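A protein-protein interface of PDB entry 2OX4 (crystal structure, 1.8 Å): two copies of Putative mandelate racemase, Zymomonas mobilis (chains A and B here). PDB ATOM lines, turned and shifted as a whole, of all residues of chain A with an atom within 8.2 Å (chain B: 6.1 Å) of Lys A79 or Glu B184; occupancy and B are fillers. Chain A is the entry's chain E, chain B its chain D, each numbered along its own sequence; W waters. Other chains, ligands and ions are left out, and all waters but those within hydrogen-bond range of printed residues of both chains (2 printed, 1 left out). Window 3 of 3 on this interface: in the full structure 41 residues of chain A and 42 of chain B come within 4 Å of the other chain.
The guanidinium group (NH1) of Arg B268 lies within hydrogen-bond range of the side-chain amide oxygen (OE1) of Gln A85, at 3.4 Å. The side-chain amide nitrogen (NE2) of Gln A85 sits at hydrogen-bond distance from the side-chain hydroxyl (OG1) of Thr B245 (2.9 Å). O of Gly B218 is in hydrogen-bond range of NE2 of Gln A85 (2.9 Å). The side-chain amino group (NZ) of Lys A79 is in salt-bridge range of the side-chain carboxylate (OE1) of Glu B184 (2.7 Å). The guanidinium group (NH1) of Arg B268 is in hydrogen-bond range of the backbone carbonyl oxygen (O) of Phe A82.
The backbone carbonyl oxygen of Lys A79 lies close to the side-chain amide oxygen of Gln A85. N of Gln A85 is in hydrogen-bond range of O of Phe A78 (3.3 Å). OE2 of Glu A75 lies within salt-bridge range of NZ of Lys A79, at 2.9 Å.
Among the printed residues, pairs that only touch across the chains: Lys A79 with Thr B245 (3.9 Å) and Trp A83 with Arg B268 (3.9 Å).
Of the printed residues of chain B, Lys A79 touches Glu B184 (2.7 Å) and Thr B245 (3.9 Å). Of the printed residues of chain B, Trp A83 touches Arg B268 (3.9 Å). Printed residues of chain A within 4 Å of Glu B184: Lys A79 (2.7 Å). Pro B186 touches none of the printed residues of chain A. Of the printed residues of chain A, Gly B218 touches Gln A85. Of the printed residues of chain A, Arg B268 touches Phe A82 (2.9 Å), Trp A83 (3.9 Å) and Gln A85 (3.4 Å). The nearest printed residue of chain B that does not touch Lys A79 is Gly B218 (5.6 Å). The nearest printed residue of chain B that does not touch Trp A83 is Thr B245 (8.4 Å).
Hydrophobic or aromatic side chains of chain A within 4 Å of the printed part of chain B: Phe A82 and Trp A83. Printed residues of chain B that touch a printed residue of chain A: Glu B184, Gly B218, Thr B245 and Arg B268. Among the printed residues, Asp or Glu carboxylates within 4 Å of a Lys or Arg side-chain nitrogen of the other chain: Lys A79 with Glu B184.
No position is printed for both chains. Of the 7 pairs that touch across the chains among the printed residues, none has its exchanged pair printed and touching as well.
Water W2 bridges the side-chain carboxylate (OE2) of Glu A75 and the side-chain carboxylate (OE2) of Glu B184. Water W1 bridges the side-chain amide oxygen (OE1) of Gln A85 (2.8 Å) and the guanidinium group (NH1) of Arg B268 (2.9 Å).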
ATOM      1  N   LEU A  61      23.556 -20.463  20.126  1.00  0.00           N
ATOM      2  CA  LEU A  61      22.183 -19.985  20.231  1.00  0.00           C
ATOM      3  C   LEU A  61      21.247 -20.773  19.322  1.00  0.00           C
ATOM      4  O   LEU A  61      20.028 -20.653  19.430  1.00  0.00           O
ATOM      5  CB  LEU A  61      22.103 -18.497  19.896  1.00  0.00           C
ATOM      6  CG  LEU A  61      22.589 -17.448  20.915  1.00  0.00           C
ATOM      7  CD1 LEU A  61      24.035 -17.655  21.315  1.00  0.00           C
ATOM      8  CD2 LEU A  61      22.409 -16.057  20.327  1.00  0.00           C
ATOM      9  N   ALA A  72      12.210 -15.433  13.283  1.00  0.00           N
ATOM     10  CA  ALA A  72      12.495 -15.361  14.720  1.00  0.00           C
ATOM     11  C   ALA A  72      13.987 -15.535  14.979  1.00  0.00           C
ATOM     12  O   ALA A  72      14.524 -14.898  15.870  1.00  0.00           O
ATOM     13  CB  ALA A  72      11.700 -16.415  15.484  1.00  0.00           C
ATOM     14  N   ILE A  73      14.653 -16.397  14.202  1.00  0.00           N
ATOM     15  CA  ILE A  73      16.062 -16.674  14.443  1.00  0.00           C
ATOM     16  C   ILE A  73      16.886 -15.436  14.033  1.00  0.00           C
ATOM     17  O   ILE A  73      17.810 -15.034  14.750  1.00  0.00           O
ATOM     18  CB  ILE A  73      16.566 -17.931  13.692  1.00  0.00           C
ATOM     19  CG1 ILE A  73      15.989 -19.216  14.312  1.00  0.00           C
ATOM     20  CG2 ILE A  73      18.103 -18.001  13.756  1.00  0.00           C
ATOM     21  CD1 ILE A  73      16.202 -20.501  13.430  1.00  0.00           C
ATOM     22  N   TRP A  74      16.538 -14.844  12.887  1.00  0.00           N
ATOM     23  CA  TRP A  74      17.184 -13.609  12.422  1.00  0.00           C
ATOM     24  C   TRP A  74      17.056 -12.545  13.526  1.00  0.00           C
ATOM     25  O   TRP A  74      18.034 -11.926  13.917  1.00  0.00           O
ATOM     26  CB  TRP A  74      16.547 -13.135  11.092  1.00  0.00           C
ATOM     27  CG  TRP A  74      17.456 -12.287  10.209  1.00  0.00           C
ATOM     28  CD1 TRP A  74      18.112 -12.691   9.062  1.00  0.00           C
ATOM     29  CD2 TRP A  74      17.795 -10.898  10.397  1.00  0.00           C
ATOM     30  NE1 TRP A  74      18.844 -11.642   8.545  1.00  0.00           N
ATOM     31  CE2 TRP A  74      18.667 -10.533   9.343  1.00  0.00           C
ATOM     32  CE3 TRP A  74      17.443  -9.928  11.353  1.00  0.00           C
ATOM     33  CZ2 TRP A  74      19.204  -9.237   9.221  1.00  0.00           C
ATOM     34  CZ3 TRP A  74      17.980  -8.630  11.236  1.00  0.00           C
ATOM     35  CH2 TRP A  74      18.848  -8.302  10.173  1.00  0.00           C
ATOM     36  N   GLU A  75      15.838 -12.364  14.038  1.00  0.00           N
ATOM     37  CA  GLU A  75      15.582 -11.327  15.037  1.00  0.00           C
ATOM     38  C   GLU A  75      16.311 -11.650  16.347  1.00  0.00           C
ATOM     39  O   GLU A  75      16.775 -10.740  17.040  1.00  0.00           O
ATOM     40  CB  GLU A  75      14.069 -11.117  15.240  1.00  0.00           C
ATOM     41  CG  GLU A  75      13.680  -9.985  16.239  1.00  0.00           C
ATOM     42  CD  GLU A  75      13.767  -8.560  15.656  1.00  0.00           C
ATOM     43  OE1 GLU A  75      14.231  -8.372  14.510  1.00  0.00           O
ATOM     44  OE2 GLU A  75      13.370  -7.616  16.381  1.00  0.00           O
ATOM     45  N   LYS A  76      16.437 -12.938  16.658  1.00  0.00           N
ATOM     46  CA  LYS A  76      17.186 -13.374  17.849  1.00  0.00           C
ATOM     47  C   LYS A  76      18.681 -13.048  17.723  1.00  0.00           C
ATOM     48  O   LYS A  76      19.292 -12.508  18.651  1.00  0.00           O
ATOM     49  CB  LYS A  76      16.998 -14.879  18.089  1.00  0.00           C
ATOM     50  CG  LYS A  76      17.793 -15.439  19.254  1.00  0.00           C
ATOM     51  CD  LYS A  76      17.493 -16.929  19.415  1.00  0.00           C
ATOM     52  CE  LYS A  76      18.451 -17.587  20.391  1.00  0.00           C
ATOM     53  NZ  LYS A  76      18.117 -19.028  20.591  1.00  0.00           N
ATOM     54  N   LEU A  77      19.279 -13.361  16.576  1.00  0.00           N
ATOM     55  CA  LEU A  77      20.682 -13.025  16.383  1.00  0.00           C
ATOM     56  C   LEU A  77      20.884 -11.504  16.313  1.00  0.00           C
ATOM     57  O   LEU A  77      21.923 -11.000  16.707  1.00  0.00           O
ATOM     58  CB  LEU A  77      21.246 -13.705  15.133  1.00  0.00           C
ATOM     59  CG  LEU A  77      21.273 -15.237  15.197  1.00  0.00           C
ATOM     60  CD1 LEU A  77      21.806 -15.788  13.872  1.00  0.00           C
ATOM     61  CD2 LEU A  77      22.159 -15.705  16.362  1.00  0.00           C
ATOM     62  N   PHE A  78      19.875 -10.781  15.835  1.00  0.00           N
ATOM     63  CA  PHE A  78      19.932  -9.318  15.798  1.00  0.00           C
ATOM     64  C   PHE A  78      19.837  -8.709  17.215  1.00  0.00           C
ATOM     65  O   PHE A  78      20.623  -7.824  17.560  1.00  0.00           O
ATOM     66  CB  PHE A  78      18.808  -8.783  14.902  1.00  0.00           C
ATOM     67  CG  PHE A  78      18.841  -7.290  14.672  1.00  0.00           C
ATOM     68  CD1 PHE A  78      20.033  -6.629  14.374  1.00  0.00           C
ATOM     69  CD2 PHE A  78      17.654  -6.553  14.715  1.00  0.00           C
ATOM     70  CE1 PHE A  78      20.039  -5.235  14.141  1.00  0.00           C
ATOM     71  CE2 PHE A  78      17.657  -5.163  14.489  1.00  0.00           C
ATOM     72  CZ  PHE A  78      18.852  -4.516  14.201  1.00  0.00           C
ATOM     73  N   LYS A  79      18.898  -9.216  18.019  1.00  0.00           N
ATOM     74  CA  LYS A  79      18.450  -8.541  19.248  1.00  0.00           C
ATOM     75  C   LYS A  79      18.988  -9.141  20.546  1.00  0.00           C
ATOM     76  O   LYS A  79      18.981  -8.471  21.593  1.00  0.00           O
ATOM     77  CB  LYS A  79      16.917  -8.486  19.312  1.00  0.00           C
ATOM     78  CG  LYS A  79      16.298  -7.572  18.247  1.00  0.00           C
ATOM     79  CD  LYS A  79      16.700  -6.121  18.476  1.00  0.00           C
ATOM     80  CE  LYS A  79      15.843  -5.169  17.630  1.00  0.00           C
ATOM     81  NZ  LYS A  79      14.353  -5.289  17.840  1.00  0.00           N
ATOM     82  N   LYS A  80      19.443 -10.389  20.488  1.00  0.00           N
ATOM     83  CA  LYS A  80      19.819 -11.117  21.706  1.00  0.00           C
ATOM     84  C   LYS A  80      21.315 -11.385  21.846  1.00  0.00           C
ATOM     85  O   LYS A  80      21.748 -11.992  22.826  1.00  0.00           O
ATOM     86  CB  LYS A  80      19.034 -12.428  21.842  1.00  0.00           C
ATOM     87  CG  LYS A  80      17.516 -12.253  21.938  1.00  0.00           C
ATOM     88  CD  LYS A  80      17.133 -11.476  23.189  1.00  0.00           C
ATOM     89  CE  LYS A  80      15.652 -11.180  23.212  1.00  0.00           C
ATOM     90  NZ  LYS A  80      15.258 -10.515  24.477  1.00  0.00           N
ATOM     91  N   THR A  81      22.107 -10.924  20.882  1.00  0.00           N
ATOM     92  CA  THR A  81      23.549 -11.146  20.915  1.00  0.00           C
ATOM     93  C   THR A  81      24.299  -9.928  21.474  1.00  0.00           C
ATOM     94  O   THR A  81      25.520  -9.983  21.699  1.00  0.00           O
ATOM     95  CB  THR A  81      24.086 -11.413  19.499  1.00  0.00           C
ATOM     96  OG1 THR A  81      23.682 -10.345  18.641  1.00  0.00           O
ATOM     97  CG2 THR A  81      23.548 -12.737  18.957  1.00  0.00           C
ATOM     98  N   PHE A  82      23.545  -8.849  21.684  1.00  0.00           N
ATOM     99  CA  PHE A  82      24.052  -7.495  22.020  1.00  0.00           C
ATOM    100  C   PHE A  82      24.692  -6.781  20.832  1.00  0.00           C
ATOM    101  O   PHE A  82      24.290  -5.676  20.474  1.00  0.00           O
ATOM    102  CB  PHE A  82      24.988  -7.456  23.246  1.00  0.00           C
ATOM    103  CG  PHE A  82      25.011  -6.108  23.909  1.00  0.00           C
ATOM    104  CD1 PHE A  82      23.987  -5.745  24.792  1.00  0.00           C
ATOM    105  CD2 PHE A  82      25.998  -5.184  23.613  1.00  0.00           C
ATOM    106  CE1 PHE A  82      23.965  -4.491  25.388  1.00  0.00           C
ATOM    107  CE2 PHE A  82      25.981  -3.897  24.208  1.00  0.00           C
ATOM    108  CZ  PHE A  82      24.961  -3.568  25.094  1.00  0.00           C
ATOM    109  N   TRP A  83      25.663  -7.430  20.202  1.00  0.00           N
ATOM    110  CA  TRP A  83      26.402  -6.810  19.110  1.00  0.00           C
ATOM    111  C   TRP A  83      25.616  -6.723  17.810  1.00  0.00           C
ATOM    112  O   TRP A  83      25.928  -5.891  16.965  1.00  0.00           O
ATOM    113  CB  TRP A  83      27.793  -7.440  18.950  1.00  0.00           C
ATOM    114  CG  TRP A  83      28.448  -7.467  20.305  1.00  0.00           C
ATOM    115  CD1 TRP A  83      28.672  -8.565  21.097  1.00  0.00           C
ATOM    116  CD2 TRP A  83      28.874  -6.328  21.062  1.00  0.00           C
ATOM    117  NE1 TRP A  83      29.227  -8.172  22.299  1.00  0.00           N
ATOM    118  CE2 TRP A  83      29.374  -6.808  22.298  1.00  0.00           C
ATOM    119  CE3 TRP A  83      28.883  -4.944  20.818  1.00  0.00           C
ATOM    120  CZ2 TRP A  83      29.877  -5.954  23.284  1.00  0.00           C
ATOM    121  CZ3 TRP A  83      29.395  -4.094  21.805  1.00  0.00           C
ATOM    122  CH2 TRP A  83      29.876  -4.603  23.020  1.00  0.00           C
ATOM    123  N   GLY A  84      24.576  -7.551  17.676  1.00  0.00           N
ATOM    124  CA  GLY A  84      23.653  -7.454  16.543  1.00  0.00           C
ATOM    125  C   GLY A  84      23.154  -6.030  16.326  1.00  0.00           C
ATOM    126  O   GLY A  84      23.141  -5.537  15.195  1.00  0.00           O
ATOM    127  N   GLN A  85      22.785  -5.350  17.417  1.00  0.00           N
ATOM    128  CA  GLN A  85      22.225  -4.006  17.311  1.00  0.00           C
ATOM    129  C   GLN A  85      23.254  -2.917  17.008  1.00  0.00           C
ATOM    130  O   GLN A  85      22.883  -1.793  16.670  1.00  0.00           O
ATOM    131  CB  GLN A  85      21.415  -3.659  18.556  1.00  0.00           C
ATOM    132  CG  GLN A  85      20.071  -4.382  18.631  1.00  0.00           C
ATOM    133  CD  GLN A  85      19.485  -4.367  20.032  1.00  0.00           C
ATOM    134  OE1 GLN A  85      19.766  -5.253  20.850  1.00  0.00           O
ATOM    135  NE2 GLN A  85      18.655  -3.373  20.315  1.00  0.00           N
ATOM    136  N   ILE A  95      24.906 -13.865  10.645  1.00  0.00           N
ATOM    137  CA  ILE A  95      23.470 -14.031  10.447  1.00  0.00           C
ATOM    138  C   ILE A  95      23.191 -14.573   9.035  1.00  0.00           C
ATOM    139  O   ILE A  95      22.398 -15.514   8.864  1.00  0.00           O
ATOM    140  CB  ILE A  95      22.703 -12.714  10.688  1.00  0.00           C
ATOM    141  CG1 ILE A  95      22.987 -12.188  12.116  1.00  0.00           C
ATOM    142  CG2 ILE A  95      21.204 -12.963  10.474  1.00  0.00           C
ATOM    143  CD1 ILE A  95      22.216 -10.926  12.507  1.00  0.00           C
ATOM    144  N   TRP A 273      19.067  -1.653   7.296  1.00  0.00           N
ATOM    145  CA  TRP A 273      19.562  -0.453   7.983  1.00  0.00           C
ATOM    146  C   TRP A 273      20.739   0.180   7.245  1.00  0.00           C
ATOM    147  O   TRP A 273      20.878   1.402   7.223  1.00  0.00           O
ATOM    148  CB  TRP A 273      19.973  -0.793   9.420  1.00  0.00           C
ATOM    149  CG  TRP A 273      18.818  -1.050  10.350  1.00  0.00           C
ATOM    150  CD1 TRP A 273      18.263  -0.161  11.216  1.00  0.00           C
ATOM    151  CD2 TRP A 273      18.105  -2.288  10.528  1.00  0.00           C
ATOM    152  NE1 TRP A 273      17.243  -0.752  11.919  1.00  0.00           N
ATOM    153  CE2 TRP A 273      17.122  -2.058  11.520  1.00  0.00           C
ATOM    154  CE3 TRP A 273      18.212  -3.570   9.959  1.00  0.00           C
ATOM    155  CZ2 TRP A 273      16.233  -3.062  11.954  1.00  0.00           C
ATOM    156  CZ3 TRP A 273      17.330  -4.570  10.380  1.00  0.00           C
ATOM    157  CH2 TRP A 273      16.349  -4.307  11.372  1.00  0.00           C
ATOM    158  N   PHE B 182       9.846  -8.341  27.568  1.00  0.00           N
ATOM    159  CA  PHE B 182       9.907  -7.785  26.223  1.00  0.00           C
ATOM    160  C   PHE B 182       9.510  -6.316  26.286  1.00  0.00           C
ATOM    161  O   PHE B 182       8.476  -5.968  26.879  1.00  0.00           O
ATOM    162  CB  PHE B 182       8.950  -8.547  25.294  1.00  0.00           C
ATOM    163  CG  PHE B 182       9.063  -8.145  23.848  1.00  0.00           C
ATOM    164  CD1 PHE B 182      10.110  -8.618  23.065  1.00  0.00           C
ATOM    165  CD2 PHE B 182       8.129  -7.285  23.275  1.00  0.00           C
ATOM    166  CE1 PHE B 182      10.223  -8.244  21.723  1.00  0.00           C
ATOM    167  CE2 PHE B 182       8.235  -6.910  21.939  1.00  0.00           C
ATOM    168  CZ  PHE B 182       9.283  -7.391  21.167  1.00  0.00           C
ATOM    169  N   LEU B 183      10.344  -5.456  25.701  1.00  0.00           N
ATOM    170  CA  LEU B 183      10.279  -4.021  25.996  1.00  0.00           C
ATOM    171  C   LEU B 183      10.164  -3.143  24.741  1.00  0.00           C
ATOM    172  O   LEU B 183      10.369  -1.927  24.799  1.00  0.00           O
ATOM    173  CB  LEU B 183      11.483  -3.592  26.856  1.00  0.00           C
ATOM    174  CG  LEU B 183      11.601  -4.306  28.218  1.00  0.00           C
ATOM    175  CD1 LEU B 183      12.980  -4.134  28.848  1.00  0.00           C
ATOM    176  CD2 LEU B 183      10.519  -3.834  29.178  1.00  0.00           C
ATOM    177  N   GLU B 184       9.828  -3.754  23.608  1.00  0.00           N
ATOM    178  CA  GLU B 184       9.611  -2.985  22.389  1.00  0.00           C
ATOM    179  C   GLU B 184       8.139  -2.652  22.196  1.00  0.00           C
ATOM    180  O   GLU B 184       7.261  -3.464  22.517  1.00  0.00           O
ATOM    181  CB  GLU B 184      10.171  -3.742  21.177  1.00  0.00           C
ATOM    182  CG  GLU B 184      11.687  -3.931  21.279  1.00  0.00           C
ATOM    183  CD  GLU B 184      12.247  -4.966  20.321  1.00  0.00           C
ATOM    184  OE1 GLU B 184      13.463  -5.224  20.399  1.00  0.00           O
ATOM    185  OE2 GLU B 184      11.491  -5.516  19.493  1.00  0.00           O
ATOM    186  N   GLY B 185       7.865  -1.459  21.668  1.00  0.00           N
ATOM    187  CA  GLY B 185       6.486  -1.036  21.416  1.00  0.00           C
ATOM    188  C   GLY B 185       5.848  -0.542  22.713  1.00  0.00           C
ATOM    189  O   GLY B 185       6.496  -0.537  23.756  1.00  0.00           O
ATOM    190  N   PRO B 186       4.578  -0.112  22.649  1.00  0.00           N
ATOM    191  CA  PRO B 186       3.914   0.414  23.842  1.00  0.00           C
ATOM    192  C   PRO B 186       3.931  -0.623  24.978  1.00  0.00           C
ATOM    193  O   PRO B 186       3.665  -1.807  24.747  1.00  0.00           O
ATOM    194  CB  PRO B 186       2.485   0.683  23.356  1.00  0.00           C
ATOM    195  CG  PRO B 186       2.604   0.894  21.889  1.00  0.00           C
ATOM    196  CD  PRO B 186       3.695  -0.080  21.468  1.00  0.00           C
ATOM    197  N   LEU B 187       4.260  -0.158  26.179  1.00  0.00           N
ATOM    198  CA  LEU B 187       4.480  -1.013  27.358  1.00  0.00           C
ATOM    199  C   LEU B 187       3.215  -1.107  28.219  1.00  0.00           C
ATOM    200  O   LEU B 187       2.463  -0.132  28.334  1.00  0.00           O
ATOM    201  CB  LEU B 187       5.596  -0.426  28.224  1.00  0.00           C
ATOM    202  CG  LEU B 187       7.018  -0.413  27.662  1.00  0.00           C
ATOM    203  CD1 LEU B 187       8.000   0.086  28.698  1.00  0.00           C
ATOM    204  CD2 LEU B 187       7.435  -1.787  27.147  1.00  0.00           C
ATOM    205  N   GLY B 218      19.463  -0.824  25.188  1.00  0.00           N
ATOM    206  CA  GLY B 218      18.842  -1.073  23.877  1.00  0.00           C
ATOM    207  C   GLY B 218      17.720  -2.111  23.861  1.00  0.00           C
ATOM    208  O   GLY B 218      17.420  -2.678  22.807  1.00  0.00           O
ATOM    209  N   HIS B 219      17.079  -2.361  25.007  1.00  0.00           N
ATOM    210  CA  HIS B 219      15.980  -3.335  25.055  1.00  0.00           C
ATOM    211  C   HIS B 219      14.669  -2.701  24.636  1.00  0.00           C
ATOM    212  O   HIS B 219      13.767  -3.387  24.159  1.00  0.00           O
ATOM    213  CB  HIS B 219      15.810  -3.946  26.450  1.00  0.00           C
ATOM    214  CG  HIS B 219      16.983  -4.756  26.907  1.00  0.00           C
ATOM    215  ND1 HIS B 219      17.368  -4.814  28.230  1.00  0.00           N
ATOM    216  CD2 HIS B 219      17.840  -5.555  26.228  1.00  0.00           C
ATOM    217  CE1 HIS B 219      18.417  -5.610  28.346  1.00  0.00           C
ATOM    218  NE2 HIS B 219      18.731  -6.063  27.145  1.00  0.00           N
ATOM    219  N   THR B 220      14.586  -1.387  24.838  1.00  0.00           N
ATOM    220  CA  THR B 220      13.435  -0.579  24.463  1.00  0.00           C
ATOM    221  C   THR B 220      13.579  -0.155  22.995  1.00  0.00           C
ATOM    222  O   THR B 220      14.618  -0.397  22.359  1.00  0.00           O
ATOM    223  CB  THR B 220      13.287   0.669  25.392  1.00  0.00           C
ATOM    224  OG1 THR B 220      14.556   1.307  25.565  1.00  0.00           O
ATOM    225  CG2 THR B 220      12.782   0.228  26.783  1.00  0.00           C
ATOM    226  N   ASP B 221      12.527   0.451  22.458  1.00  0.00           N
ATOM    227  CA  ASP B 221      12.662   1.205  21.217  1.00  0.00           C
ATOM    228  C   ASP B 221      12.176   2.625  21.461  1.00  0.00           C
ATOM    229  O   ASP B 221      11.864   2.990  22.597  1.00  0.00           O
ATOM    230  CB  ASP B 221      11.919   0.524  20.049  1.00  0.00           C
ATOM    231  CG  ASP B 221      10.425   0.359  20.299  1.00  0.00           C
ATOM    232  OD1 ASP B 221       9.852   1.083  21.146  1.00  0.00           O
ATOM    233  OD2 ASP B 221       9.814  -0.502  19.627  1.00  0.00           O
ATOM    234  N   SER B 224       8.597   2.837  23.470  1.00  0.00           N
ATOM    235  CA  SER B 224       8.705   2.487  24.881  1.00  0.00           C
ATOM    236  C   SER B 224       9.679   3.394  25.657  1.00  0.00           C
ATOM    237  O   SER B 224       9.443   3.698  26.833  1.00  0.00           O
ATOM    238  CB  SER B 224       9.044   1.009  25.039  1.00  0.00           C
ATOM    239  OG  SER B 224      10.271   0.695  24.382  1.00  0.00           O
ATOM    240  N   THR B 245      17.656   0.933  19.370  1.00  0.00           N
ATOM    241  CA  THR B 245      18.678   0.379  18.482  1.00  0.00           C
ATOM    242  C   THR B 245      19.379   1.531  17.743  1.00  0.00           C
ATOM    243  O   THR B 245      18.709   2.379  17.166  1.00  0.00           O
ATOM    244  CB  THR B 245      18.014  -0.595  17.506  1.00  0.00           C
ATOM    245  OG1 THR B 245      17.498  -1.702  18.262  1.00  0.00           O
ATOM    246  CG2 THR B 245      19.020  -1.116  16.448  1.00  0.00           C
ATOM    247  N   ARG B 268      27.682   0.952  21.339  1.00  0.00           N
ATOM    248  CA  ARG B 268      27.412   0.240  20.078  1.00  0.00           C
ATOM    249  C   ARG B 268      27.432   1.167  18.874  1.00  0.00           C
ATOM    250  O   ARG B 268      26.694   0.954  17.913  1.00  0.00           O
ATOM    251  CB  ARG B 268      26.109  -0.556  20.154  1.00  0.00           C
ATOM    252  CG  ARG B 268      26.277  -1.872  20.942  1.00  0.00           C
ATOM    253  CD  ARG B 268      24.974  -2.651  20.989  1.00  0.00           C
ATOM    254  NE  ARG B 268      24.049  -2.073  21.969  1.00  0.00           N
ATOM    255  CZ  ARG B 268      22.986  -2.700  22.461  1.00  0.00           C
ATOM    256  NH1 ARG B 268      22.700  -3.950  22.093  1.00  0.00           N
ATOM    257  NH2 ARG B 268      22.229  -2.081  23.370  1.00  0.00           N
HETATM  258  O   HOH W   1      20.438  -5.076  23.545  1.00  0.00           O
HETATM  259  O   HOH W   2      12.092  -8.080  18.707  1.00  0.00           O
